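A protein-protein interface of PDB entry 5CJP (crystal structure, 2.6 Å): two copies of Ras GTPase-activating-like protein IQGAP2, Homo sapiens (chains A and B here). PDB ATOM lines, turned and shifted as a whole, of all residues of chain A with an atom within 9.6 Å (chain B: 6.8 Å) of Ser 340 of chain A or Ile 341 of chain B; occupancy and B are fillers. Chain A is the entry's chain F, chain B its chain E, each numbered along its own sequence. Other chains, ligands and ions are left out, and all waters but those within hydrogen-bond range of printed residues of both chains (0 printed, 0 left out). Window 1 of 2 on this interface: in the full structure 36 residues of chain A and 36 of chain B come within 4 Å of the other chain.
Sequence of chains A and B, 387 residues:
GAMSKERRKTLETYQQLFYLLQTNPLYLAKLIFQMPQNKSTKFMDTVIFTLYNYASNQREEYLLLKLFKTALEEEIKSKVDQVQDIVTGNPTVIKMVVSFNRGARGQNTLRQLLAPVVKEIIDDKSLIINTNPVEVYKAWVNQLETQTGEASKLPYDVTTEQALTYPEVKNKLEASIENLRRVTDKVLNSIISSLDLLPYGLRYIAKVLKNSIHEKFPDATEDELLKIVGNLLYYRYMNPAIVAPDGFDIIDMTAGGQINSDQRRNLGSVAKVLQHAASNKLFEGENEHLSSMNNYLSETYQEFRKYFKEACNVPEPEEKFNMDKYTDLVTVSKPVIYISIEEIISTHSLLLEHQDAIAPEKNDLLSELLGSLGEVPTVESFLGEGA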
ATOM      1  N   LEU A  11      -7.694   8.880   3.392  1.00  0.00           N
ATOM      2  CA  LEU A  11      -6.786   8.140   2.521  1.00  0.00           C
ATOM      3  C   LEU A  11      -5.894   9.048   1.668  1.00  0.00           C
ATOM      4  O   LEU A  11      -4.684   8.821   1.554  1.00  0.00           O
ATOM      5  CB  LEU A  11      -7.577   7.198   1.609  1.00  0.00           C
ATOM      6  CG  LEU A  11      -6.720   6.544   0.532  1.00  0.00           C
ATOM      7  CD1 LEU A  11      -5.760   5.567   1.176  1.00  0.00           C
ATOM      8  CD2 LEU A  11      -7.606   5.833  -0.489  1.00  0.00           C
ATOM      9  N   TYR A  14      -3.083  10.866   3.840  1.00  0.00           N
ATOM     10  CA  TYR A  14      -1.887  10.079   4.061  1.00  0.00           C
ATOM     11  C   TYR A  14      -1.162   9.906   2.744  1.00  0.00           C
ATOM     12  O   TYR A  14       0.069   9.950   2.711  1.00  0.00           O
ATOM     13  CB  TYR A  14      -2.231   8.691   4.595  1.00  0.00           C
ATOM     14  CG  TYR A  14      -2.530   8.648   6.059  1.00  0.00           C
ATOM     15  CD1 TYR A  14      -1.518   8.419   6.987  1.00  0.00           C
ATOM     16  CD2 TYR A  14      -3.829   8.805   6.518  1.00  0.00           C
ATOM     17  CE1 TYR A  14      -1.806   8.349   8.349  1.00  0.00           C
ATOM     18  CE2 TYR A  14      -4.124   8.734   7.862  1.00  0.00           C
ATOM     19  CZ  TYR A  14      -3.116   8.502   8.780  1.00  0.00           C
ATOM     20  OH  TYR A  14      -3.441   8.412  10.121  1.00  0.00           O
ATOM     21  N   GLN A  15      -1.914   9.695   1.666  1.00  0.00           N
ATOM     22  CA  GLN A  15      -1.293   9.490   0.351  1.00  0.00           C
ATOM     23  C   GLN A  15      -0.435  10.683  -0.050  1.00  0.00           C
ATOM     24  O   GLN A  15       0.712  10.517  -0.448  1.00  0.00           O
ATOM     25  CB  GLN A  15      -2.346   9.190  -0.738  1.00  0.00           C
ATOM     26  CG  GLN A  15      -2.948   7.797  -0.608  1.00  0.00           C
ATOM     27  CD  GLN A  15      -3.923   7.438  -1.717  1.00  0.00           C
ATOM     28  OE1 GLN A  15      -4.832   8.212  -2.049  1.00  0.00           O
ATOM     29  NE2 GLN A  15      -3.750   6.245  -2.287  1.00  0.00           N
ATOM     30  N   GLN A  16      -0.993  11.879   0.068  1.00  0.00           N
ATOM     31  CA  GLN A  16      -0.257  13.082  -0.254  1.00  0.00           C
ATOM     32  C   GLN A  16       0.934  13.218   0.710  1.00  0.00           C
ATOM     33  O   GLN A  16       2.100  13.318   0.292  1.00  0.00           O
ATOM     34  CB  GLN A  16      -1.188  14.291  -0.145  1.00  0.00           C
ATOM     35  CG  GLN A  16      -2.132  14.452  -1.337  1.00  0.00           C
ATOM     36  CD  GLN A  16      -1.370  14.521  -2.649  1.00  0.00           C
ATOM     37  OE1 GLN A  16      -0.396  15.268  -2.766  1.00  0.00           O
ATOM     38  NE2 GLN A  16      -1.803  13.744  -3.637  1.00  0.00           N
ATOM     39  N   LEU A  17       0.632  13.188   2.004  1.00  0.00           N
ATOM     40  CA  LEU A  17       1.652  13.307   3.046  1.00  0.00           C
ATOM     41  C   LEU A  17       2.910  12.453   2.823  1.00  0.00           C
ATOM     42  O   LEU A  17       4.026  12.974   2.840  1.00  0.00           O
ATOM     43  CB  LEU A  17       1.035  12.980   4.410  1.00  0.00           C
ATOM     44  CG  LEU A  17       1.990  13.110   5.603  1.00  0.00           C
ATOM     45  CD1 LEU A  17       2.640  14.500   5.604  1.00  0.00           C
ATOM     46  CD2 LEU A  17       1.236  12.881   6.896  1.00  0.00           C
ATOM     47  N   PHE A  18       2.750  11.148   2.607  1.00  0.00           N
ATOM     48  CA  PHE A  18       3.933  10.298   2.422  1.00  0.00           C
ATOM     49  C   PHE A  18       4.553  10.378   1.037  1.00  0.00           C
ATOM     50  O   PHE A  18       5.686   9.953   0.823  1.00  0.00           O
ATOM     51  CB  PHE A  18       3.622   8.851   2.855  1.00  0.00           C
ATOM     52  CG  PHE A  18       3.661   8.664   4.373  1.00  0.00           C
ATOM     53  CD1 PHE A  18       4.894   8.576   5.055  1.00  0.00           C
ATOM     54  CD2 PHE A  18       2.485   8.695   5.129  1.00  0.00           C
ATOM     55  CE1 PHE A  18       4.954   8.529   6.465  1.00  0.00           C
ATOM     56  CE2 PHE A  18       2.531   8.649   6.542  1.00  0.00           C
ATOM     57  CZ  PHE A  18       3.773   8.567   7.205  1.00  0.00           C
ATOM     58  N   TYR A  19       3.808  10.953   0.103  1.00  0.00           N
ATOM     59  CA  TYR A  19       4.315  11.164  -1.242  1.00  0.00           C
ATOM     60  C   TYR A  19       5.265  12.386  -1.136  1.00  0.00           C
ATOM     61  O   TYR A  19       6.423  12.344  -1.567  1.00  0.00           O
ATOM     62  CB  TYR A  19       3.155  11.474  -2.202  1.00  0.00           C
ATOM     63  CG  TYR A  19       3.607  12.097  -3.508  1.00  0.00           C
ATOM     64  CD1 TYR A  19       4.435  11.397  -4.388  1.00  0.00           C
ATOM     65  CD2 TYR A  19       3.245  13.411  -3.839  1.00  0.00           C
ATOM     66  CE1 TYR A  19       4.894  11.989  -5.563  1.00  0.00           C
ATOM     67  CE2 TYR A  19       3.697  14.017  -5.011  1.00  0.00           C
ATOM     68  CZ  TYR A  19       4.516  13.304  -5.862  1.00  0.00           C
ATOM     69  OH  TYR A  19       4.962  13.894  -7.019  1.00  0.00           O
ATOM     70  N   LEU A  20       4.753  13.461  -0.545  1.00  0.00           N
ATOM     71  CA  LEU A  20       5.520  14.684  -0.357  1.00  0.00           C
ATOM     72  C   LEU A  20       6.751  14.505   0.538  1.00  0.00           C
ATOM     73  O   LEU A  20       7.810  15.058   0.259  1.00  0.00           O
ATOM     74  CB  LEU A  20       4.618  15.776   0.223  1.00  0.00           C
ATOM     75  CG  LEU A  20       3.568  16.233  -0.791  1.00  0.00           C
ATOM     76  CD1 LEU A  20       2.838  17.451  -0.256  1.00  0.00           C
ATOM     77  CD2 LEU A  20       4.260  16.586  -2.117  1.00  0.00           C
ATOM     78  N   GLN A  22       8.665  11.919   0.962  1.00  0.00           N
ATOM     79  CA  GLN A  22       9.759  11.265   0.246  1.00  0.00           C
ATOM     80  C   GLN A  22      10.334  12.063  -0.917  1.00  0.00           C
ATOM     81  O   GLN A  22      11.554  12.139  -1.093  1.00  0.00           O
ATOM     82  CB  GLN A  22       9.308   9.915  -0.303  1.00  0.00           C
ATOM     83  CG  GLN A  22       8.913   8.908   0.761  1.00  0.00           C
ATOM     84  CD  GLN A  22       8.116   7.755   0.185  1.00  0.00           C
ATOM     85  OE1 GLN A  22       8.657   6.862  -0.476  1.00  0.00           O
ATOM     86  NE2 GLN A  22       6.819   7.780   0.414  1.00  0.00           N
ATOM     87  N   THR A  23       9.447  12.660  -1.702  1.00  0.00           N
ATOM     88  CA  THR A  23       9.849  13.360  -2.907  1.00  0.00           C
ATOM     89  C   THR A  23       9.975  14.871  -2.881  1.00  0.00           C
ATOM     90  O   THR A  23      10.668  15.444  -3.713  1.00  0.00           O
ATOM     91  CB  THR A  23       8.893  13.026  -4.054  1.00  0.00           C
ATOM     92  OG1 THR A  23       7.567  13.398  -3.676  1.00  0.00           O
ATOM     93  CG2 THR A  23       8.923  11.560  -4.367  1.00  0.00           C
ATOM     94  N   VAL A 336      11.187   9.647 -10.633  1.00  0.00           N
ATOM     95  CA  VAL A 336      11.196   9.226  -9.237  1.00  0.00           C
ATOM     96  C   VAL A 336      10.224   8.098  -8.863  1.00  0.00           C
ATOM     97  O   VAL A 336       9.030   8.148  -9.169  1.00  0.00           O
ATOM     98  CB  VAL A 336      10.927  10.434  -8.303  1.00  0.00           C
ATOM     99  CG1 VAL A 336      11.942  11.530  -8.576  1.00  0.00           C
ATOM    100  CG2 VAL A 336       9.519  10.961  -8.505  1.00  0.00           C
ATOM    101  N   ILE A 337      10.774   7.078  -8.208  1.00  0.00           N
ATOM    102  CA  ILE A 337      10.008   5.934  -7.722  1.00  0.00           C
ATOM    103  C   ILE A 337       9.826   6.197  -6.247  1.00  0.00           C
ATOM    104  O   ILE A 337      10.777   6.534  -5.559  1.00  0.00           O
ATOM    105  CB  ILE A 337      10.789   4.606  -7.882  1.00  0.00           C
ATOM    106  CG1 ILE A 337      10.607   4.053  -9.291  1.00  0.00           C
ATOM    107  CG2 ILE A 337      10.310   3.583  -6.904  1.00  0.00           C
ATOM    108  CD1 ILE A 337      11.240   4.919 -10.337  1.00  0.00           C
ATOM    109  N   TYR A 338       8.607   6.072  -5.748  1.00  0.00           N
ATOM    110  CA  TYR A 338       8.388   6.283  -4.324  1.00  0.00           C
ATOM    111  C   TYR A 338       7.430   5.232  -3.754  1.00  0.00           C
ATOM    112  O   TYR A 338       6.716   4.550  -4.499  1.00  0.00           O
ATOM    113  CB  TYR A 338       7.843   7.688  -4.072  1.00  0.00           C
ATOM    114  CG  TYR A 338       6.460   7.876  -4.619  1.00  0.00           C
ATOM    115  CD1 TYR A 338       5.344   7.806  -3.780  1.00  0.00           C
ATOM    116  CD2 TYR A 338       6.252   8.074  -5.989  1.00  0.00           C
ATOM    117  CE1 TYR A 338       4.051   7.923  -4.290  1.00  0.00           C
ATOM    118  CE2 TYR A 338       4.962   8.197  -6.512  1.00  0.00           C
ATOM    119  CZ  TYR A 338       3.868   8.121  -5.652  1.00  0.00           C
ATOM    120  OH  TYR A 338       2.593   8.248  -6.162  1.00  0.00           O
ATOM    121  N   ILE A 339       7.443   5.100  -2.431  1.00  0.00           N
ATOM    122  CA  ILE A 339       6.573   4.158  -1.734  1.00  0.00           C
ATOM    123  C   ILE A 339       5.225   4.829  -1.519  1.00  0.00           C
ATOM    124  O   ILE A 339       5.156   5.919  -0.980  1.00  0.00           O
ATOM    125  CB  ILE A 339       7.169   3.726  -0.373  1.00  0.00           C
ATOM    126  CG1 ILE A 339       8.295   2.707  -0.606  1.00  0.00           C
ATOM    127  CG2 ILE A 339       6.096   3.097   0.498  1.00  0.00           C
ATOM    128  CD1 ILE A 339       7.842   1.517  -1.333  1.00  0.00           C
ATOM    129  N   SER A 340       4.154   4.169  -1.950  1.00  0.00           N
ATOM    130  CA  SER A 340       2.803   4.716  -1.839  1.00  0.00           C
ATOM    131  C   SER A 340       1.807   3.835  -1.096  1.00  0.00           C
ATOM    132  O   SER A 340       1.975   2.611  -1.014  1.00  0.00           O
ATOM    133  CB  SER A 340       2.254   4.956  -3.234  1.00  0.00           C
ATOM    134  OG  SER A 340       2.321   3.745  -3.962  1.00  0.00           O
ATOM    135  N   ILE A 341       0.764   4.482  -0.576  1.00  0.00           N
ATOM    136  CA  ILE A 341      -0.315   3.802   0.108  1.00  0.00           C
ATOM    137  C   ILE A 341      -1.458   3.661  -0.936  1.00  0.00           C
ATOM    138  O   ILE A 341      -1.768   4.601  -1.673  1.00  0.00           O
ATOM    139  CB  ILE A 341      -0.723   4.564   1.433  1.00  0.00           C
ATOM    140  CG1 ILE A 341      -2.210   4.817   1.476  1.00  0.00           C
ATOM    141  CG2 ILE A 341       0.078   5.789   1.624  1.00  0.00           C
ATOM    142  CD1 ILE A 341      -2.971   3.573   1.578  1.00  0.00           C
ATOM    143  N   GLU A 342      -2.026   2.463  -1.048  1.00  0.00           N
ATOM    144  CA  GLU A 342      -3.084   2.190  -2.019  1.00  0.00           C
ATOM    145  C   GLU A 342      -4.303   1.563  -1.342  1.00  0.00           C
ATOM    146  O   GLU A 342      -4.177   0.943  -0.287  1.00  0.00           O
ATOM    147  CB  GLU A 342      -2.569   1.217  -3.083  1.00  0.00           C
ATOM    148  CG  GLU A 342      -1.191   1.525  -3.628  1.00  0.00           C
ATOM    149  CD  GLU A 342      -1.198   2.658  -4.646  1.00  0.00           C
ATOM    150  OE1 GLU A 342      -2.292   3.002  -5.160  1.00  0.00           O
ATOM    151  OE2 GLU A 342      -0.103   3.194  -4.945  1.00  0.00           O
ATOM    152  N   GLU A 343      -5.476   1.729  -1.945  1.00  0.00           N
ATOM    153  CA  GLU A 343      -6.715   1.139  -1.415  1.00  0.00           C
ATOM    154  C   GLU A 343      -7.197   0.112  -2.436  1.00  0.00           C
ATOM    155  O   GLU A 343      -6.891   0.219  -3.621  1.00  0.00           O
ATOM    156  CB  GLU A 343      -7.815   2.202  -1.233  1.00  0.00           C
ATOM    157  CG  GLU A 343      -8.664   2.474  -2.507  1.00  0.00           C
ATOM    158  CD  GLU A 343      -9.796   3.508  -2.301  1.00  0.00           C
ATOM    159  OE1 GLU A 343     -10.652   3.290  -1.417  1.00  0.00           O
ATOM    160  OE2 GLU A 343      -9.838   4.536  -3.028  1.00  0.00           O
ATOM    161  N   LEU A 373      12.539 -10.360 -11.627  1.00  0.00           N
ATOM    162  CA  LEU A 373      12.800  -9.155 -10.848  1.00  0.00           C
ATOM    163  C   LEU A 373      14.283  -8.967 -10.544  1.00  0.00           C
ATOM    164  O   LEU A 373      14.804  -9.540  -9.581  1.00  0.00           O
ATOM    165  CB  LEU A 373      12.031  -9.218  -9.527  1.00  0.00           C
ATOM    166  CG  LEU A 373      10.549  -9.564  -9.634  1.00  0.00           C
ATOM    167  CD1 LEU A 373       9.973  -9.726  -8.243  1.00  0.00           C
ATOM    168  CD2 LEU A 373       9.816  -8.483 -10.406  1.00  0.00           C
ATOM    169  N   LEU B  11       7.667  -2.571 -12.824  1.00  0.00           N
ATOM    170  CA  LEU B  11       7.135  -1.823 -11.696  1.00  0.00           C
ATOM    171  C   LEU B  11       5.822  -2.470 -11.258  1.00  0.00           C
ATOM    172  O   LEU B  11       5.511  -2.547 -10.065  1.00  0.00           O
ATOM    173  CB  LEU B  11       6.877  -0.362 -12.090  1.00  0.00           C
ATOM    174  CG  LEU B  11       6.471   0.494 -10.890  1.00  0.00           C
ATOM    175  CD1 LEU B  11       7.700   0.763 -10.077  1.00  0.00           C
ATOM    176  CD2 LEU B  11       5.837   1.783 -11.321  1.00  0.00           C
ATOM    177  N   TYR B  14       6.344  -5.600  -9.363  1.00  0.00           N
ATOM    178  CA  TYR B  14       6.782  -5.303  -7.996  1.00  0.00           C
ATOM    179  C   TYR B  14       5.596  -4.901  -7.134  1.00  0.00           C
ATOM    180  O   TYR B  14       5.513  -5.297  -5.970  1.00  0.00           O
ATOM    181  CB  TYR B  14       7.827  -4.185  -7.989  1.00  0.00           C
ATOM    182  CG  TYR B  14       9.249  -4.690  -7.970  1.00  0.00           C
ATOM    183  CD1 TYR B  14       9.821  -5.152  -6.792  1.00  0.00           C
ATOM    184  CD2 TYR B  14      10.007  -4.749  -9.142  1.00  0.00           C
ATOM    185  CE1 TYR B  14      11.111  -5.666  -6.769  1.00  0.00           C
ATOM    186  CE2 TYR B  14      11.303  -5.262  -9.140  1.00  0.00           C
ATOM    187  CZ  TYR B  14      11.854  -5.725  -7.949  1.00  0.00           C
ATOM    188  OH  TYR B  14      13.132  -6.266  -7.927  1.00  0.00           O
ATOM    189  N   GLN B  15       4.681  -4.120  -7.704  1.00  0.00           N
ATOM    190  CA  GLN B  15       3.490  -3.683  -6.978  1.00  0.00           C
ATOM    191  C   GLN B  15       2.648  -4.906  -6.607  1.00  0.00           C
ATOM    192  O   GLN B  15       2.058  -4.970  -5.526  1.00  0.00           O
ATOM    193  CB  GLN B  15       2.663  -2.722  -7.842  1.00  0.00           C
ATOM    194  CG  GLN B  15       3.422  -1.500  -8.339  1.00  0.00           C
ATOM    195  CD  GLN B  15       2.570  -0.612  -9.244  1.00  0.00           C
ATOM    196  OE1 GLN B  15       1.949  -1.093 -10.191  1.00  0.00           O
ATOM    197  NE2 GLN B  15       2.542   0.687  -8.954  1.00  0.00           N
ATOM    198  N   PHE B  18       4.227  -6.572  -3.653  1.00  0.00           N
ATOM    199  CA  PHE B  18       3.942  -5.888  -2.411  1.00  0.00           C
ATOM    200  C   PHE B  18       2.505  -6.098  -1.970  1.00  0.00           C
ATOM    201  O   PHE B  18       2.225  -6.262  -0.792  1.00  0.00           O
ATOM    202  CB  PHE B  18       4.282  -4.412  -2.569  1.00  0.00           C
ATOM    203  CG  PHE B  18       5.744  -4.165  -2.762  1.00  0.00           C
ATOM    204  CD1 PHE B  18       6.639  -5.228  -2.849  1.00  0.00           C
ATOM    205  CD2 PHE B  18       6.236  -2.873  -2.816  1.00  0.00           C
ATOM    206  CE1 PHE B  18       8.001  -5.009  -2.981  1.00  0.00           C
ATOM    207  CE2 PHE B  18       7.601  -2.643  -2.948  1.00  0.00           C
ATOM    208  CZ  PHE B  18       8.486  -3.712  -3.030  1.00  0.00           C
ATOM    209  N   TYR B 338      -3.007  -0.797   1.617  1.00  0.00           N
ATOM    210  CA  TYR B 338      -1.693  -1.420   1.608  1.00  0.00           C
ATOM    211  C   TYR B 338      -0.583  -0.508   1.081  1.00  0.00           C
ATOM    212  O   TYR B 338      -0.823   0.549   0.511  1.00  0.00           O
ATOM    213  CB  TYR B 338      -1.728  -2.730   0.821  1.00  0.00           C
ATOM    214  CG  TYR B 338      -1.903  -2.567  -0.676  1.00  0.00           C
ATOM    215  CD1 TYR B 338      -0.822  -2.738  -1.553  1.00  0.00           C
ATOM    216  CD2 TYR B 338      -3.160  -2.268  -1.226  1.00  0.00           C
ATOM    217  CE1 TYR B 338      -0.995  -2.612  -2.931  1.00  0.00           C
ATOM    218  CE2 TYR B 338      -3.337  -2.146  -2.596  1.00  0.00           C
ATOM    219  CZ  TYR B 338      -2.260  -2.318  -3.440  1.00  0.00           C
ATOM    220  OH  TYR B 338      -2.447  -2.200  -4.801  1.00  0.00           O
ATOM    221  N   ILE B 339       0.644  -0.956   1.258  1.00  0.00           N
ATOM    222  CA  ILE B 339       1.816  -0.206   0.868  1.00  0.00           C
ATOM    223  C   ILE B 339       2.407  -0.695  -0.448  1.00  0.00           C
ATOM    224  O   ILE B 339       2.763  -1.868  -0.577  1.00  0.00           O
ATOM    225  CB  ILE B 339       2.856  -0.341   1.986  1.00  0.00           C
ATOM    226  CG1 ILE B 339       2.342   0.407   3.228  1.00  0.00           C
ATOM    227  CG2 ILE B 339       4.225   0.063   1.500  1.00  0.00           C
ATOM    228  CD1 ILE B 339       2.094   1.856   2.999  1.00  0.00           C
ATOM    229  N   SER B 340       2.546   0.196  -1.422  1.00  0.00           N
ATOM    230  CA  SER B 340       3.095  -0.214  -2.715  1.00  0.00           C
ATOM    231  C   SER B 340       4.174   0.757  -3.249  1.00  0.00           C
ATOM    232  O   SER B 340       4.588   1.699  -2.566  1.00  0.00           O
ATOM    233  CB  SER B 340       1.926  -0.340  -3.718  1.00  0.00           C
ATOM    234  OG  SER B 340       2.307  -1.022  -4.915  1.00  0.00           O
ATOM    235  N   ILE B 341       4.622   0.511  -4.472  1.00  0.00           N
ATOM    236  CA  ILE B 341       5.608   1.348  -5.138  1.00  0.00           C
ATOM    237  C   ILE B 341       4.858   2.078  -6.246  1.00  0.00           C
ATOM    238  O   ILE B 341       3.828   1.598  -6.713  1.00  0.00           O
ATOM    239  CB  ILE B 341       6.691   0.510  -5.803  1.00  0.00           C
ATOM    240  CG1 ILE B 341       7.659  -0.028  -4.777  1.00  0.00           C
ATOM    241  CG2 ILE B 341       7.493   1.344  -6.768  1.00  0.00           C
ATOM    242  CD1 ILE B 341       8.618  -0.966  -5.431  1.00  0.00           C
ATOM    243  N   GLU B 342       5.372   3.234  -6.662  1.00  0.00           N
ATOM    244  CA  GLU B 342       4.760   4.019  -7.731  1.00  0.00           C
ATOM    245  C   GLU B 342       5.788   4.951  -8.367  1.00  0.00           C
ATOM    246  O   GLU B 342       6.655   5.494  -7.686  1.00  0.00           O
ATOM    247  CB  GLU B 342       3.581   4.839  -7.201  1.00  0.00           C
ATOM    248  CG  GLU B 342       2.748   5.463  -8.315  1.00  0.00           C
ATOM    249  CD  GLU B 342       2.138   4.415  -9.258  1.00  0.00           C
ATOM    250  OE1 GLU B 342       1.104   3.813  -8.878  1.00  0.00           O
ATOM    251  OE2 GLU B 342       2.697   4.182 -10.368  1.00  0.00           O
ATOM    252  N   GLU B 343       5.709   5.126  -9.678  1.00  0.00           N
ATOM    253  CA  GLU B 343       6.651   6.001 -10.357  1.00  0.00           C
ATOM    254  C   GLU B 343       5.914   7.283 -10.698  1.00  0.00           C
ATOM    255  O   GLU B 343       4.726   7.249 -11.006  1.00  0.00           O
ATOM    256  CB  GLU B 343       7.202   5.325 -11.615  1.00  0.00           C
ATOM    257  CG  GLU B 343       8.352   6.080 -12.269  1.00  0.00           C
ATOM    258  CD  GLU B 343       8.946   5.352 -13.464  1.00  0.00           C
ATOM    259  OE1 GLU B 343       9.575   4.289 -13.268  1.00  0.00           O
ATOM    260  OE2 GLU B 343       8.782   5.847 -14.603  1.00  0.00           O
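Tyr 338 of chain A touches Glu 342 of chain B, and with the chains exchanged Glu 342 of chain A touches Tyr 338 of chain B. Ile 339 of chain B touches its own counterpart, Ile 339 of chain A. Ile 339 of chain A touches Ser 340 of chain B, and with the chains exchanged Ser 340 of chain A touches Ile 339 of chain B. Ser 340 of chain A touches Glu 342 of chain B, and with the chains exchanged Glu 342 of chain A touches Ser 340 of chain B. Of the 19 pairs that touch across the chains among the printed residues, 10 have their exchanged pair printed and touching as well.
Printed residues of chain B that touch a printed residue of chain A: Tyr 14, Tyr 338, Ile 339, Ser 340, Ile 341, Glu 342 and Glu 343. Of the 19 printed residues of chain A, 8 touch a printed residue of chain B. Among the printed residues, 19 pairs touch across the chains.
The backbone NH (N) of Tyr 338 of chain A is in hydrogen-bond range of the backbone carbonyl oxygen (O) of Glu 342 of chain B, 2.8 Å away. The backbone carbonyl oxygen (O) of Ser 340 of chain A sits at hydrogen-bond distance from the backbone NH (N) of Ser 340 of chain B, 2.5 Å away. The backbone carbonyl oxygen (O) of Tyr 338 of chain B is in hydrogen-bond range of the backbone NH (N) of Glu 342 of chain A (2.7 Å).
Ile 341 of chain B touches just these residues of chain A: Ile 337, Tyr 338, Ile 339 and Ser 340. Of chain A, only Ile 339, Ser 340 and Glu 342 come within 4 Å of Ser 340 of chain B. Glu 342 of chain B touches just these residues of chain A: Val 336 (3.9 Å), Ile 337 (3.4 Å), Tyr 338 (2.8 Å) and Ser 340 (3.6 Å). Of the printed residues of chain A, Tyr 338 of chain B touches Ser 340, Ile 341 and Glu 342. Of the printed residues of chain B, Leu 373 of chain A touches Tyr 14 (3.5 Å). Printed residues of chain B within 4 Å of Glu 342 of chain A: Tyr 338 and Ser 340. Of the printed residues of chain B, Ile 341 of chain A touches Tyr 338. Printed residues of chain B within 4 Å of Ile 337 of chain A: Ile 341, Glu 342 and Glu 343. Leu 17 of chain A touches none of the printed residues of chain B. The nearest residue of chain B that does not touch Ser 340 of chain A is Gln 15 of chain B (5.9 Å). The nearest printed residue of chain A that does not touch Tyr 338 of chain B is Glu 343 of chain A (4.4 Å).
Among the printed residues, merely in contact across the chains: Val 336 of chain A with Glu 342 of chain B, Val 336 of chain A with Glu 343 of chain B, Ile 337 of chain A with Ile 341 of chain B, Ile 337 of chain A with Glu 342 of chain B, Ile 337 of chain A with Glu 343 of chain B, Tyr 338 of chain A with Ile 341 of chain B, Ile 339 of chain A with Ile 339 of chain B, Ile 339 of chain A with Ser 340 of chain B, Ile 339 of chain A with Ile 341 of chain B, Ser 340 of chain A with Tyr 338 of chain B, Ser 340 of chain A with Ile 339 of chain B, Ser 340 of chain A with Ile 341 of chain B, Ser 340 of chain A with Glu 342 of chain B, Ile 341 of chain A with Tyr 338 of chain B, Glu 342 of chain A with Ser 340 of chain B and Leu 373 of chain A with Tyr 14 of chain B.
The side-chain amide nitrogen (NE2) of Gln 15 of chain B is in hydrogen-bond range of the side-chain carboxylate (OE1) of Glu 342 of chain B, 3.4 Å away. O of Ile 339 of chain A lies within hydrogen-bond range of NE2 of Gln 22 of chain A (2.9 Å). NE2 of Gln 15 of chain A sits at hydrogen-bond distance from O of Ile 341 of chain A (2.6 Å). The side-chain carboxylate (OE2) of Glu 342 of chain A sits at hydrogen-bond distance from the side-chain hydroxyl (OG) of Ser 340 of chain A (2.7 Å). The side-chain amide nitrogen (NE2) of Gln 15 of chain B sits at hydrogen-bond distance from the backbone carbonyl oxygen (O) of Ile 341 of chain B (2.7 Å).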
